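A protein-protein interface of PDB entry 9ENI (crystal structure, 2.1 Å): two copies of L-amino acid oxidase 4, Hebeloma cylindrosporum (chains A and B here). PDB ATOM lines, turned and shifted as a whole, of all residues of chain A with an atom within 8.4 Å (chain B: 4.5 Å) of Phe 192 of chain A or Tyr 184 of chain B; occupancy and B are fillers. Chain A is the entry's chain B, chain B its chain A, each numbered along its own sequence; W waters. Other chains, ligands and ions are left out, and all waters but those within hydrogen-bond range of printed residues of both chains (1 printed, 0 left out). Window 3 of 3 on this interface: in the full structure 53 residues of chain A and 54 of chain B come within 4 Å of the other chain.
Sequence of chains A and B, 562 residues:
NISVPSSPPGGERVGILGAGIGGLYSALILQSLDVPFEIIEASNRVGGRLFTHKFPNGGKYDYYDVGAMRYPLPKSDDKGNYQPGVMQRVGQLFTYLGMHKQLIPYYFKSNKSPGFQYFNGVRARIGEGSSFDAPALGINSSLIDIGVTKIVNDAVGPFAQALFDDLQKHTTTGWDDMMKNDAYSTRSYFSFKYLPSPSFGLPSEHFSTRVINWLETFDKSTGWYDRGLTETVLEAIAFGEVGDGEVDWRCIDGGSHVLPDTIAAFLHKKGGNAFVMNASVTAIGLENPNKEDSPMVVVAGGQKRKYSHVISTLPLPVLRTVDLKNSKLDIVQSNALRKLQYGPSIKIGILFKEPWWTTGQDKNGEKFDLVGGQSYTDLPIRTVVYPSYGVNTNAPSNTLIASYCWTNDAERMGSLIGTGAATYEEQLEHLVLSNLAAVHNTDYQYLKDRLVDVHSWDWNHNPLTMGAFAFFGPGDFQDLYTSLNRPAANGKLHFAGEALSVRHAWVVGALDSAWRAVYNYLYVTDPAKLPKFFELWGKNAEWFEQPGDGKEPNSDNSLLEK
The backbone NH (N) of Leu 229 of chain B sits at hydrogen-bond distance from the backbone carbonyl oxygen (O) of Tyr 184 of chain B (2.9 Å).
The side-chain hydroxyl (OG) of Ser 185 of chain B is in hydrogen-bond range of the backbone NH (N) of Ser 188 of chain B (2.9 Å).
The backbone NH of Arg 187 of chain A sits close to the side-chain hydroxyl of Ser 185 of chain A (3.5 Å).
The side-chain hydroxyl (OG) of Ser 185 of chain A lies within hydrogen-bond range of the backbone NH (N) of Ser 188 of chain A.
The backbone carbonyl oxygen (O) of Arg 187 of chain A lies within hydrogen-bond range of the side-chain hydroxyl (OG) of Ser 191 of chain A, 3.3 Å away.
The backbone carbonyl oxygen (O) of Phe 192 of chain A lies within hydrogen-bond range of a ring nitrogen (NE2) of His 206 of chain A, at 3.4 Å.
Among the printed residues, merely in contact across the chains: Phe 192 of chain A with Tyr 184 of chain B, Asp 226 of chain A with Pro 474 of chain B, Arg 187 of chain A with Pro 474 of chain B, Phe 192 of chain A with Ala 183 of chain B, Ser 191 of chain A with Ala 183 of chain B and Ser 188 of chain A with Ser 188 of chain B.
Of the printed residues of chain B, Ser 191 of chain A touches Ala 183 (3.7 Å).
Of the printed residues of chain B, Phe 192 of chain A touches Ala 183 and Tyr 184.
Lys 193 of chain A touches none of the printed residues of chain B.
Printed residues of chain B within 4 Å of Asp 226 of chain A: Pro 474.
Of chain A, only Phe 192 (3.2 Å) comes within 4 Å of Tyr 184 of chain B.
Of the printed residues of chain A, Ser 188 of chain B touches Ser 188.
Of the printed residues of chain A, Pro 474 of chain B touches Arg 187 and Asp 226.
The nearest residue of chain B that does not touch Phe 192 of chain A is Ser 188 of chain B (4.4 Å).
The nearest residue of chain A that does not touch Tyr 184 of chain B is Ser 188 of chain A (6.1 Å).
The nearest printed residue of chain A that does not touch Pro 474 of chain B is Thr 209 of chain A (4.9 Å).
Of the 18 printed residues of chain A, 5 touch a printed residue of chain B.
Printed residues of chain A that touch a printed residue of chain B: Arg 187, Ser 188, Ser 191, Phe 192 and Asp 226.
Hydrophobic or aromatic side chains of chain A that line the printed part of chain B: Phe 192.
Ser 188 of chain B touches its own counterpart, Ser 188 of chain A.
6 positions are printed for both chains.
Of the 6 pairs that touch across the chains among the printed residues, 1 has its exchanged pair printed and touching as well.
Water W1 lies within hydrogen-bond range of OD2 of Asp 226 of chain A (2.7 Å), O of Pro 474 of chain B (2.8 Å) and NE of Arg 187 of chain A (3.5 Å).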
ATOM      1  N   TYR A 184      19.453  22.799   8.441  1.00  0.00           N
ATOM      2  CA  TYR A 184      18.078  22.414   8.172  1.00  0.00           C
ATOM      3  C   TYR A 184      17.816  22.385   6.672  1.00  0.00           C
ATOM      4  O   TYR A 184      18.232  23.284   5.936  1.00  0.00           O
ATOM      5  CB  TYR A 184      17.086  23.394   8.818  1.00  0.00           C
ATOM      6  CG  TYR A 184      16.926  23.259  10.318  1.00  0.00           C
ATOM      7  CD1 TYR A 184      16.243  22.182  10.867  1.00  0.00           C
ATOM      8  CD2 TYR A 184      17.441  24.219  11.184  1.00  0.00           C
ATOM      9  CE1 TYR A 184      16.092  22.052  12.240  1.00  0.00           C
ATOM     10  CE2 TYR A 184      17.294  24.097  12.561  1.00  0.00           C
ATOM     11  CZ  TYR A 184      16.618  23.010  13.077  1.00  0.00           C
ATOM     12  OH  TYR A 184      16.468  22.877  14.436  1.00  0.00           O
ATOM     13  N   SER A 185      17.137  21.339   6.224  1.00  0.00           N
ATOM     14  CA  SER A 185      16.347  21.456   5.013  1.00  0.00           C
ATOM     15  C   SER A 185      15.038  22.159   5.365  1.00  0.00           C
ATOM     16  O   SER A 185      14.663  22.263   6.536  1.00  0.00           O
ATOM     17  CB  SER A 185      16.065  20.086   4.413  1.00  0.00           C
ATOM     18  OG  SER A 185      15.224  19.338   5.276  1.00  0.00           O
ATOM     19  N   THR A 186      14.320  22.627   4.344  1.00  0.00           N
ATOM     20  CA  THR A 186      13.005  23.206   4.606  1.00  0.00           C
ATOM     21  C   THR A 186      12.112  22.201   5.321  1.00  0.00           C
ATOM     22  O   THR A 186      11.392  22.557   6.260  1.00  0.00           O
ATOM     23  CB  THR A 186      12.353  23.676   3.304  1.00  0.00           C
ATOM     24  OG1 THR A 186      13.197  24.636   2.656  1.00  0.00           O
ATOM     25  CG2 THR A 186      10.979  24.297   3.564  1.00  0.00           C
ATOM     26  N   ARG A 187      12.173  20.935   4.905  1.00  0.00           N
ATOM     27  CA  ARG A 187      11.362  19.896   5.529  1.00  0.00           C
ATOM     28  C   ARG A 187      11.741  19.696   6.993  1.00  0.00           C
ATOM     29  O   ARG A 187      10.874  19.689   7.876  1.00  0.00           O
ATOM     30  CB  ARG A 187      11.522  18.587   4.750  1.00  0.00           C
ATOM     31  CG  ARG A 187      10.910  17.375   5.423  1.00  0.00           C
ATOM     32  CD  ARG A 187      11.121  16.120   4.601  1.00  0.00           C
ATOM     33  NE  ARG A 187      10.592  16.276   3.253  1.00  0.00           N
ATOM     34  CZ  ARG A 187       9.306  16.184   2.944  1.00  0.00           C
ATOM     35  NH1 ARG A 187       8.392  15.932   3.867  1.00  0.00           N
ATOM     36  NH2 ARG A 187       8.929  16.353   1.680  1.00  0.00           N
ATOM     37  N   SER A 188      13.030  19.495   7.269  1.00  0.00           N
ATOM     38  CA  SER A 188      13.433  19.230   8.645  1.00  0.00           C
ATOM     39  C   SER A 188      13.211  20.454   9.522  1.00  0.00           C
ATOM     40  O   SER A 188      12.990  20.318  10.731  1.00  0.00           O
ATOM     41  CB  SER A 188      14.892  18.775   8.698  1.00  0.00           C
ATOM     42  OG  SER A 188      15.772  19.850   8.441  1.00  0.00           O
ATOM     43  N   TYR A 189      13.239  21.652   8.935  1.00  0.00           N
ATOM     44  CA  TYR A 189      12.877  22.840   9.698  1.00  0.00           C
ATOM     45  C   TYR A 189      11.413  22.780  10.122  1.00  0.00           C
ATOM     46  O   TYR A 189      11.079  23.051  11.282  1.00  0.00           O
ATOM     47  CB  TYR A 189      13.151  24.104   8.886  1.00  0.00           C
ATOM     48  CG  TYR A 189      12.853  25.353   9.677  1.00  0.00           C
ATOM     49  CD1 TYR A 189      13.668  25.729  10.740  1.00  0.00           C
ATOM     50  CD2 TYR A 189      11.744  26.139   9.386  1.00  0.00           C
ATOM     51  CE1 TYR A 189      13.399  26.862  11.481  1.00  0.00           C
ATOM     52  CE2 TYR A 189      11.467  27.277  10.123  1.00  0.00           C
ATOM     53  CZ  TYR A 189      12.296  27.630  11.168  1.00  0.00           C
ATOM     54  OH  TYR A 189      12.030  28.758  11.906  1.00  0.00           O
ATOM     55  N   PHE A 190      10.520  22.417   9.192  1.00  0.00           N
ATOM     56  CA  PHE A 190       9.112  22.258   9.546  1.00  0.00           C
ATOM     57  C   PHE A 190       8.898  21.078  10.490  1.00  0.00           C
ATOM     58  O   PHE A 190       8.034  21.142  11.373  1.00  0.00           O
ATOM     59  CB  PHE A 190       8.254  22.079   8.287  1.00  0.00           C
ATOM     60  CG  PHE A 190       7.846  23.375   7.635  1.00  0.00           C
ATOM     61  CD1 PHE A 190       7.025  24.273   8.297  1.00  0.00           C
ATOM     62  CD2 PHE A 190       8.264  23.683   6.352  1.00  0.00           C
ATOM     63  CE1 PHE A 190       6.645  25.460   7.700  1.00  0.00           C
ATOM     64  CE2 PHE A 190       7.886  24.872   5.748  1.00  0.00           C
ATOM     65  CZ  PHE A 190       7.072  25.760   6.424  1.00  0.00           C
ATOM     66  N   SER A 191       9.674  20.004  10.340  1.00  0.00           N
ATOM     67  CA  SER A 191       9.411  18.805  11.127  1.00  0.00           C
ATOM     68  C   SER A 191       9.913  18.914  12.560  1.00  0.00           C
ATOM     69  O   SER A 191       9.348  18.274  13.454  1.00  0.00           O
ATOM     70  CB  SER A 191      10.044  17.579  10.468  1.00  0.00           C
ATOM     71  OG  SER A 191       9.309  17.178   9.331  1.00  0.00           O
ATOM     72  N   PHE A 192      10.968  19.694  12.804  1.00  0.00           N
ATOM     73  CA  PHE A 192      11.649  19.665  14.090  1.00  0.00           C
ATOM     74  C   PHE A 192      11.847  21.022  14.752  1.00  0.00           C
ATOM     75  O   PHE A 192      12.298  21.053  15.901  1.00  0.00           O
ATOM     76  CB  PHE A 192      13.014  18.982  13.939  1.00  0.00           C
ATOM     77  CG  PHE A 192      12.938  17.620  13.311  1.00  0.00           C
ATOM     78  CD1 PHE A 192      12.380  16.559  14.000  1.00  0.00           C
ATOM     79  CD2 PHE A 192      13.402  17.407  12.024  1.00  0.00           C
ATOM     80  CE1 PHE A 192      12.302  15.305  13.423  1.00  0.00           C
ATOM     81  CE2 PHE A 192      13.328  16.152  11.440  1.00  0.00           C
ATOM     82  CZ  PHE A 192      12.779  15.103  12.139  1.00  0.00           C
ATOM     83  N   LYS A 193      11.522  22.132  14.088  1.00  0.00           N
ATOM     84  CA  LYS A 193      11.786  23.443  14.669  1.00  0.00           C
ATOM     85  C   LYS A 193      10.599  24.391  14.551  1.00  0.00           C
ATOM     86  O   LYS A 193      10.170  24.973  15.552  1.00  0.00           O
ATOM     87  CB  LYS A 193      13.012  24.071  13.998  1.00  0.00           C
ATOM     88  CG  LYS A 193      13.475  25.369  14.633  1.00  0.00           C
ATOM     89  CD  LYS A 193      13.978  25.145  16.050  1.00  0.00           C
ATOM     90  CE  LYS A 193      14.638  26.394  16.607  1.00  0.00           C
ATOM     91  NZ  LYS A 193      15.116  26.181  18.001  1.00  0.00           N
ATOM     92  N   TYR A 194      10.068  24.571  13.347  1.00  0.00           N
ATOM     93  CA  TYR A 194       9.020  25.563  13.158  1.00  0.00           C
ATOM     94  C   TYR A 194       7.804  25.241  14.019  1.00  0.00           C
ATOM     95  O   TYR A 194       7.353  24.093  14.075  1.00  0.00           O
ATOM     96  CB  TYR A 194       8.616  25.647  11.690  1.00  0.00           C
ATOM     97  CG  TYR A 194       7.408  26.525  11.461  1.00  0.00           C
ATOM     98  CD1 TYR A 194       7.520  27.909  11.448  1.00  0.00           C
ATOM     99  CD2 TYR A 194       6.153  25.968  11.261  1.00  0.00           C
ATOM    100  CE1 TYR A 194       6.406  28.716  11.241  1.00  0.00           C
ATOM    101  CE2 TYR A 194       5.042  26.759  11.052  1.00  0.00           C
ATOM    102  CZ  TYR A 194       5.172  28.129  11.042  1.00  0.00           C
ATOM    103  OH  TYR A 194       4.053  28.907  10.835  1.00  0.00           O
ATOM    104  N   LEU A 195       7.275  26.262  14.688  1.00  0.00           N
ATOM    105  CA  LEU A 195       5.993  26.163  15.366  1.00  0.00           C
ATOM    106  C   LEU A 195       5.088  27.284  14.875  1.00  0.00           C
ATOM    107  O   LEU A 195       5.530  28.432  14.748  1.00  0.00           O
ATOM    108  CB  LEU A 195       6.146  26.234  16.890  1.00  0.00           C
ATOM    109  CG  LEU A 195       6.834  25.012  17.503  1.00  0.00           C
ATOM    110  CD1 LEU A 195       7.132  25.222  18.987  1.00  0.00           C
ATOM    111  CD2 LEU A 195       5.981  23.763  17.283  1.00  0.00           C
ATOM    112  N   GLU A 205       2.555  22.733  17.810  1.00  0.00           N
ATOM    113  CA  GLU A 205       3.337  21.539  17.530  1.00  0.00           C
ATOM    114  C   GLU A 205       3.798  21.579  16.080  1.00  0.00           C
ATOM    115  O   GLU A 205       3.220  22.275  15.240  1.00  0.00           O
ATOM    116  CB  GLU A 205       2.535  20.263  17.814  1.00  0.00           C
ATOM    117  CG  GLU A 205       1.301  20.092  16.949  1.00  0.00           C
ATOM    118  CD  GLU A 205       0.351  19.026  17.485  1.00  0.00           C
ATOM    119  OE1 GLU A 205       0.576  18.535  18.613  1.00  0.00           O
ATOM    120  OE2 GLU A 205      -0.625  18.682  16.780  1.00  0.00           O
ATOM    121  N   HIS A 206       4.857  20.828  15.798  1.00  0.00           N
ATOM    122  CA  HIS A 206       5.408  20.807  14.454  1.00  0.00           C
ATOM    123  C   HIS A 206       4.441  20.130  13.491  1.00  0.00           C
ATOM    124  O   HIS A 206       3.720  19.195  13.850  1.00  0.00           O
ATOM    125  CB  HIS A 206       6.750  20.078  14.437  1.00  0.00           C
ATOM    126  CG  HIS A 206       7.719  20.577  15.461  1.00  0.00           C
ATOM    127  ND1 HIS A 206       8.153  21.884  15.499  1.00  0.00           N
ATOM    128  CD2 HIS A 206       8.342  19.944  16.484  1.00  0.00           C
ATOM    129  CE1 HIS A 206       8.998  22.035  16.503  1.00  0.00           C
ATOM    130  NE2 HIS A 206       9.131  20.873  17.116  1.00  0.00           N
ATOM    131  N   PHE A 207       4.444  20.607  12.252  1.00  0.00           N
ATOM    132  CA  PHE A 207       3.572  20.041  11.236  1.00  0.00           C
ATOM    133  C   PHE A 207       3.953  18.588  10.975  1.00  0.00           C
ATOM    134  O   PHE A 207       5.121  18.201  11.068  1.00  0.00           O
ATOM    135  CB  PHE A 207       3.686  20.828   9.929  1.00  0.00           C
ATOM    136  CG  PHE A 207       3.082  22.202   9.980  1.00  0.00           C
ATOM    137  CD1 PHE A 207       2.004  22.486  10.799  1.00  0.00           C
ATOM    138  CD2 PHE A 207       3.608  23.218   9.198  1.00  0.00           C
ATOM    139  CE1 PHE A 207       1.460  23.755  10.832  1.00  0.00           C
ATOM    140  CE2 PHE A 207       3.070  24.486   9.230  1.00  0.00           C
ATOM    141  CZ  PHE A 207       1.994  24.756  10.050  1.00  0.00           C
ATOM    142  N   THR A 209       4.402  15.279   8.441  1.00  0.00           N
ATOM    143  CA  THR A 209       4.901  15.106   7.081  1.00  0.00           C
ATOM    144  C   THR A 209       3.781  15.271   6.061  1.00  0.00           C
ATOM    145  O   THR A 209       3.990  15.841   4.983  1.00  0.00           O
ATOM    146  CB  THR A 209       5.563  13.734   6.937  1.00  0.00           C
ATOM    147  OG1 THR A 209       6.768  13.697   7.713  1.00  0.00           O
ATOM    148  CG2 THR A 209       5.872  13.422   5.480  1.00  0.00           C
ATOM    149  N   ILE A 212       3.352  18.887   5.637  1.00  0.00           N
ATOM    150  CA  ILE A 212       4.534  19.456   4.994  1.00  0.00           C
ATOM    151  C   ILE A 212       4.547  19.122   3.506  1.00  0.00           C
ATOM    152  O   ILE A 212       4.897  19.964   2.668  1.00  0.00           O
ATOM    153  CB  ILE A 212       5.816  18.965   5.699  1.00  0.00           C
ATOM    154  CG1 ILE A 212       5.892  19.532   7.120  1.00  0.00           C
ATOM    155  CG2 ILE A 212       7.058  19.344   4.896  1.00  0.00           C
ATOM    156  CD1 ILE A 212       6.967  18.892   7.992  1.00  0.00           C
ATOM    157  N   ASP A 226      13.580  19.056   0.510  1.00  0.00           N
ATOM    158  CA  ASP A 226      14.699  18.265   1.008  1.00  0.00           C
ATOM    159  C   ASP A 226      16.044  18.932   0.765  1.00  0.00           C
ATOM    160  O   ASP A 226      17.066  18.440   1.258  1.00  0.00           O
ATOM    161  CB  ASP A 226      14.695  16.874   0.372  1.00  0.00           C
ATOM    162  CG  ASP A 226      13.673  15.954   1.000  1.00  0.00           C
ATOM    163  OD1 ASP A 226      13.222  16.248   2.128  1.00  0.00           O
ATOM    164  OD2 ASP A 226      13.333  14.930   0.373  1.00  0.00           O
ATOM    165  N   ASN B 181      11.067   8.261  13.458  1.00  0.00           N
ATOM    166  CA  ASN B 181      12.221   9.057  13.060  1.00  0.00           C
ATOM    167  C   ASN B 181      12.335   9.227  11.550  1.00  0.00           C
ATOM    168  O   ASN B 181      13.385   9.661  11.063  1.00  0.00           O
ATOM    169  CB  ASN B 181      13.503   8.423  13.597  1.00  0.00           C
ATOM    170  CG  ASN B 181      13.556   8.411  15.101  1.00  0.00           C
ATOM    171  OD1 ASN B 181      14.057   9.346  15.722  1.00  0.00           O
ATOM    172  ND2 ASN B 181      13.046   7.343  15.702  1.00  0.00           N
ATOM    173  N   ASP B 182      11.286   8.895  10.796  1.00  0.00           N
ATOM    174  CA  ASP B 182      11.390   8.882   9.342  1.00  0.00           C
ATOM    175  C   ASP B 182      11.446  10.277   8.744  1.00  0.00           C
ATOM    176  O   ASP B 182      11.885  10.429   7.598  1.00  0.00           O
ATOM    177  CB  ASP B 182      10.214   8.108   8.751  1.00  0.00           C
ATOM    178  CG  ASP B 182      10.315   7.957   7.256  1.00  0.00           C
ATOM    179  OD1 ASP B 182      11.313   7.368   6.781  1.00  0.00           O
ATOM    180  OD2 ASP B 182       9.390   8.430   6.563  1.00  0.00           O
ATOM    181  N   ALA B 183      11.009  11.297   9.481  1.00  0.00           N
ATOM    182  CA  ALA B 183      11.132  12.663   8.992  1.00  0.00           C
ATOM    183  C   ALA B 183      12.582  13.131   8.948  1.00  0.00           C
ATOM    184  O   ALA B 183      12.860  14.166   8.335  1.00  0.00           O
ATOM    185  CB  ALA B 183      10.293  13.608   9.855  1.00  0.00           C
ATOM    186  N   TYR B 184      13.504  12.394   9.566  1.00  0.00           N
ATOM    187  CA  TYR B 184      14.917  12.736   9.504  1.00  0.00           C
ATOM    188  C   TYR B 184      15.535  12.244   8.202  1.00  0.00           C
ATOM    189  O   TYR B 184      15.293  11.112   7.769  1.00  0.00           O
ATOM    190  CB  TYR B 184      15.690  12.116  10.674  1.00  0.00           C
ATOM    191  CG  TYR B 184      15.460  12.778  12.012  1.00  0.00           C
ATOM    192  CD1 TYR B 184      15.992  14.028  12.294  1.00  0.00           C
ATOM    193  CD2 TYR B 184      14.720  12.144  13.000  1.00  0.00           C
ATOM    194  CE1 TYR B 184      15.781  14.634  13.513  1.00  0.00           C
ATOM    195  CE2 TYR B 184      14.505  12.741  14.225  1.00  0.00           C
ATOM    196  CZ  TYR B 184      15.042  13.984  14.478  1.00  0.00           C
ATOM    197  OH  TYR B 184      14.829  14.582  15.700  1.00  0.00           O
ATOM    198  N   SER B 185      16.342  13.098   7.584  1.00  0.00           N
ATOM    199  CA  SER B 185      17.379  12.600   6.700  1.00  0.00           C
ATOM    200  C   SER B 185      18.537  12.101   7.557  1.00  0.00           C
ATOM    201  O   SER B 185      18.614  12.378   8.756  1.00  0.00           O
ATOM    202  CB  SER B 185      17.855  13.688   5.745  1.00  0.00           C
ATOM    203  OG  SER B 185      18.505  14.727   6.457  1.00  0.00           O
ATOM    204  N   THR B 186      19.451  11.353   6.945  1.00  0.00           N
ATOM    205  CA  THR B 186      20.635  10.960   7.698  1.00  0.00           C
ATOM    206  C   THR B 186      21.359  12.195   8.219  1.00  0.00           C
ATOM    207  O   THR B 186      21.787  12.233   9.379  1.00  0.00           O
ATOM    208  CB  THR B 186      21.556  10.107   6.832  1.00  0.00           C
ATOM    209  OG1 THR B 186      20.820   8.990   6.316  1.00  0.00           O
ATOM    210  CG2 THR B 186      22.738   9.584   7.655  1.00  0.00           C
ATOM    211  N   SER B 188      20.106  15.372   8.827  1.00  0.00           N
ATOM    212  CA  SER B 188      19.409  16.092   9.886  1.00  0.00           C
ATOM    213  C   SER B 188      19.376  15.276  11.172  1.00  0.00           C
ATOM    214  O   SER B 188      19.339  15.853  12.265  1.00  0.00           O
ATOM    215  CB  SER B 188      17.994  16.465   9.445  1.00  0.00           C
ATOM    216  OG  SER B 188      17.150  15.331   9.404  1.00  0.00           O
ATOM    217  N   TYR B 189      19.423  13.945  11.074  1.00  0.00           N
ATOM    218  CA  TYR B 189      19.548  13.130  12.279  1.00  0.00           C
ATOM    219  C   TYR B 189      20.888  13.386  12.965  1.00  0.00           C
ATOM    220  O   TYR B 189      20.950  13.555  14.189  1.00  0.00           O
ATOM    221  CB  TYR B 189      19.381  11.644  11.946  1.00  0.00           C
ATOM    222  CG  TYR B 189      19.435  10.741  13.165  1.00  0.00           C
ATOM    223  CD1 TYR B 189      18.401  10.735  14.098  1.00  0.00           C
ATOM    224  CD2 TYR B 189      20.518   9.894  13.382  1.00  0.00           C
ATOM    225  CE1 TYR B 189      18.449   9.918  15.217  1.00  0.00           C
ATOM    226  CE2 TYR B 189      20.574   9.073  14.499  1.00  0.00           C
ATOM    227  CZ  TYR B 189      19.536   9.093  15.412  1.00  0.00           C
ATOM    228  OH  TYR B 189      19.571   8.284  16.525  1.00  0.00           O
ATOM    229  N   LYS B 193      19.900  15.316  16.298  1.00  0.00           N
ATOM    230  CA  LYS B 193      19.463  14.314  17.261  1.00  0.00           C
ATOM    231  C   LYS B 193      20.598  13.427  17.758  1.00  0.00           C
ATOM    232  O   LYS B 193      20.761  13.256  18.969  1.00  0.00           O
ATOM    233  CB  LYS B 193      18.353  13.446  16.662  1.00  0.00           C
ATOM    234  CG  LYS B 193      17.728  12.511  17.685  1.00  0.00           C
ATOM    235  CD  LYS B 193      16.384  11.979  17.224  1.00  0.00           C
ATOM    236  CE  LYS B 193      15.785  11.043  18.267  1.00  0.00           C
ATOM    237  NZ  LYS B 193      14.571  10.339  17.759  1.00  0.00           N
ATOM    238  N   GLY B 228      16.321   9.897   3.078  1.00  0.00           N
ATOM    239  CA  GLY B 228      15.771   9.482   4.355  1.00  0.00           C
ATOM    240  C   GLY B 228      16.773   8.687   5.174  1.00  0.00           C
ATOM    241  O   GLY B 228      17.485   7.823   4.657  1.00  0.00           O
ATOM    242  N   LEU B 229      16.804   8.977   6.479  1.00  0.00           N
ATOM    243  CA  LEU B 229      17.558   8.145   7.410  1.00  0.00           C
ATOM    244  C   LEU B 229      17.130   6.688   7.296  1.00  0.00           C
ATOM    245  O   LEU B 229      17.956   5.774   7.403  1.00  0.00           O
ATOM    246  CB  LEU B 229      17.350   8.646   8.843  1.00  0.00           C
ATOM    247  CG  LEU B 229      17.862   7.781   9.998  1.00  0.00           C
ATOM    248  CD1 LEU B 229      19.384   7.742  10.013  1.00  0.00           C
ATOM    249  CD2 LEU B 229      17.318   8.278  11.333  1.00  0.00           C
ATOM    250  N   PRO B 474      13.079  11.789   3.227  1.00  0.00           N
ATOM    251  CA  PRO B 474      12.484  11.780   4.569  1.00  0.00           C
ATOM    252  C   PRO B 474      10.975  11.918   4.493  1.00  0.00           C
ATOM    253  O   PRO B 474      10.449  12.748   3.749  1.00  0.00           O
ATOM    254  CB  PRO B 474      13.122  12.994   5.254  1.00  0.00           C
ATOM    255  CG  PRO B 474      14.368  13.272   4.481  1.00  0.00           C
ATOM    256  CD  PRO B 474      14.095  12.844   3.071  1.00  0.00           C
HETATM  257  O   HOH W   1      11.164  13.533   1.175  1.00  0.00           O
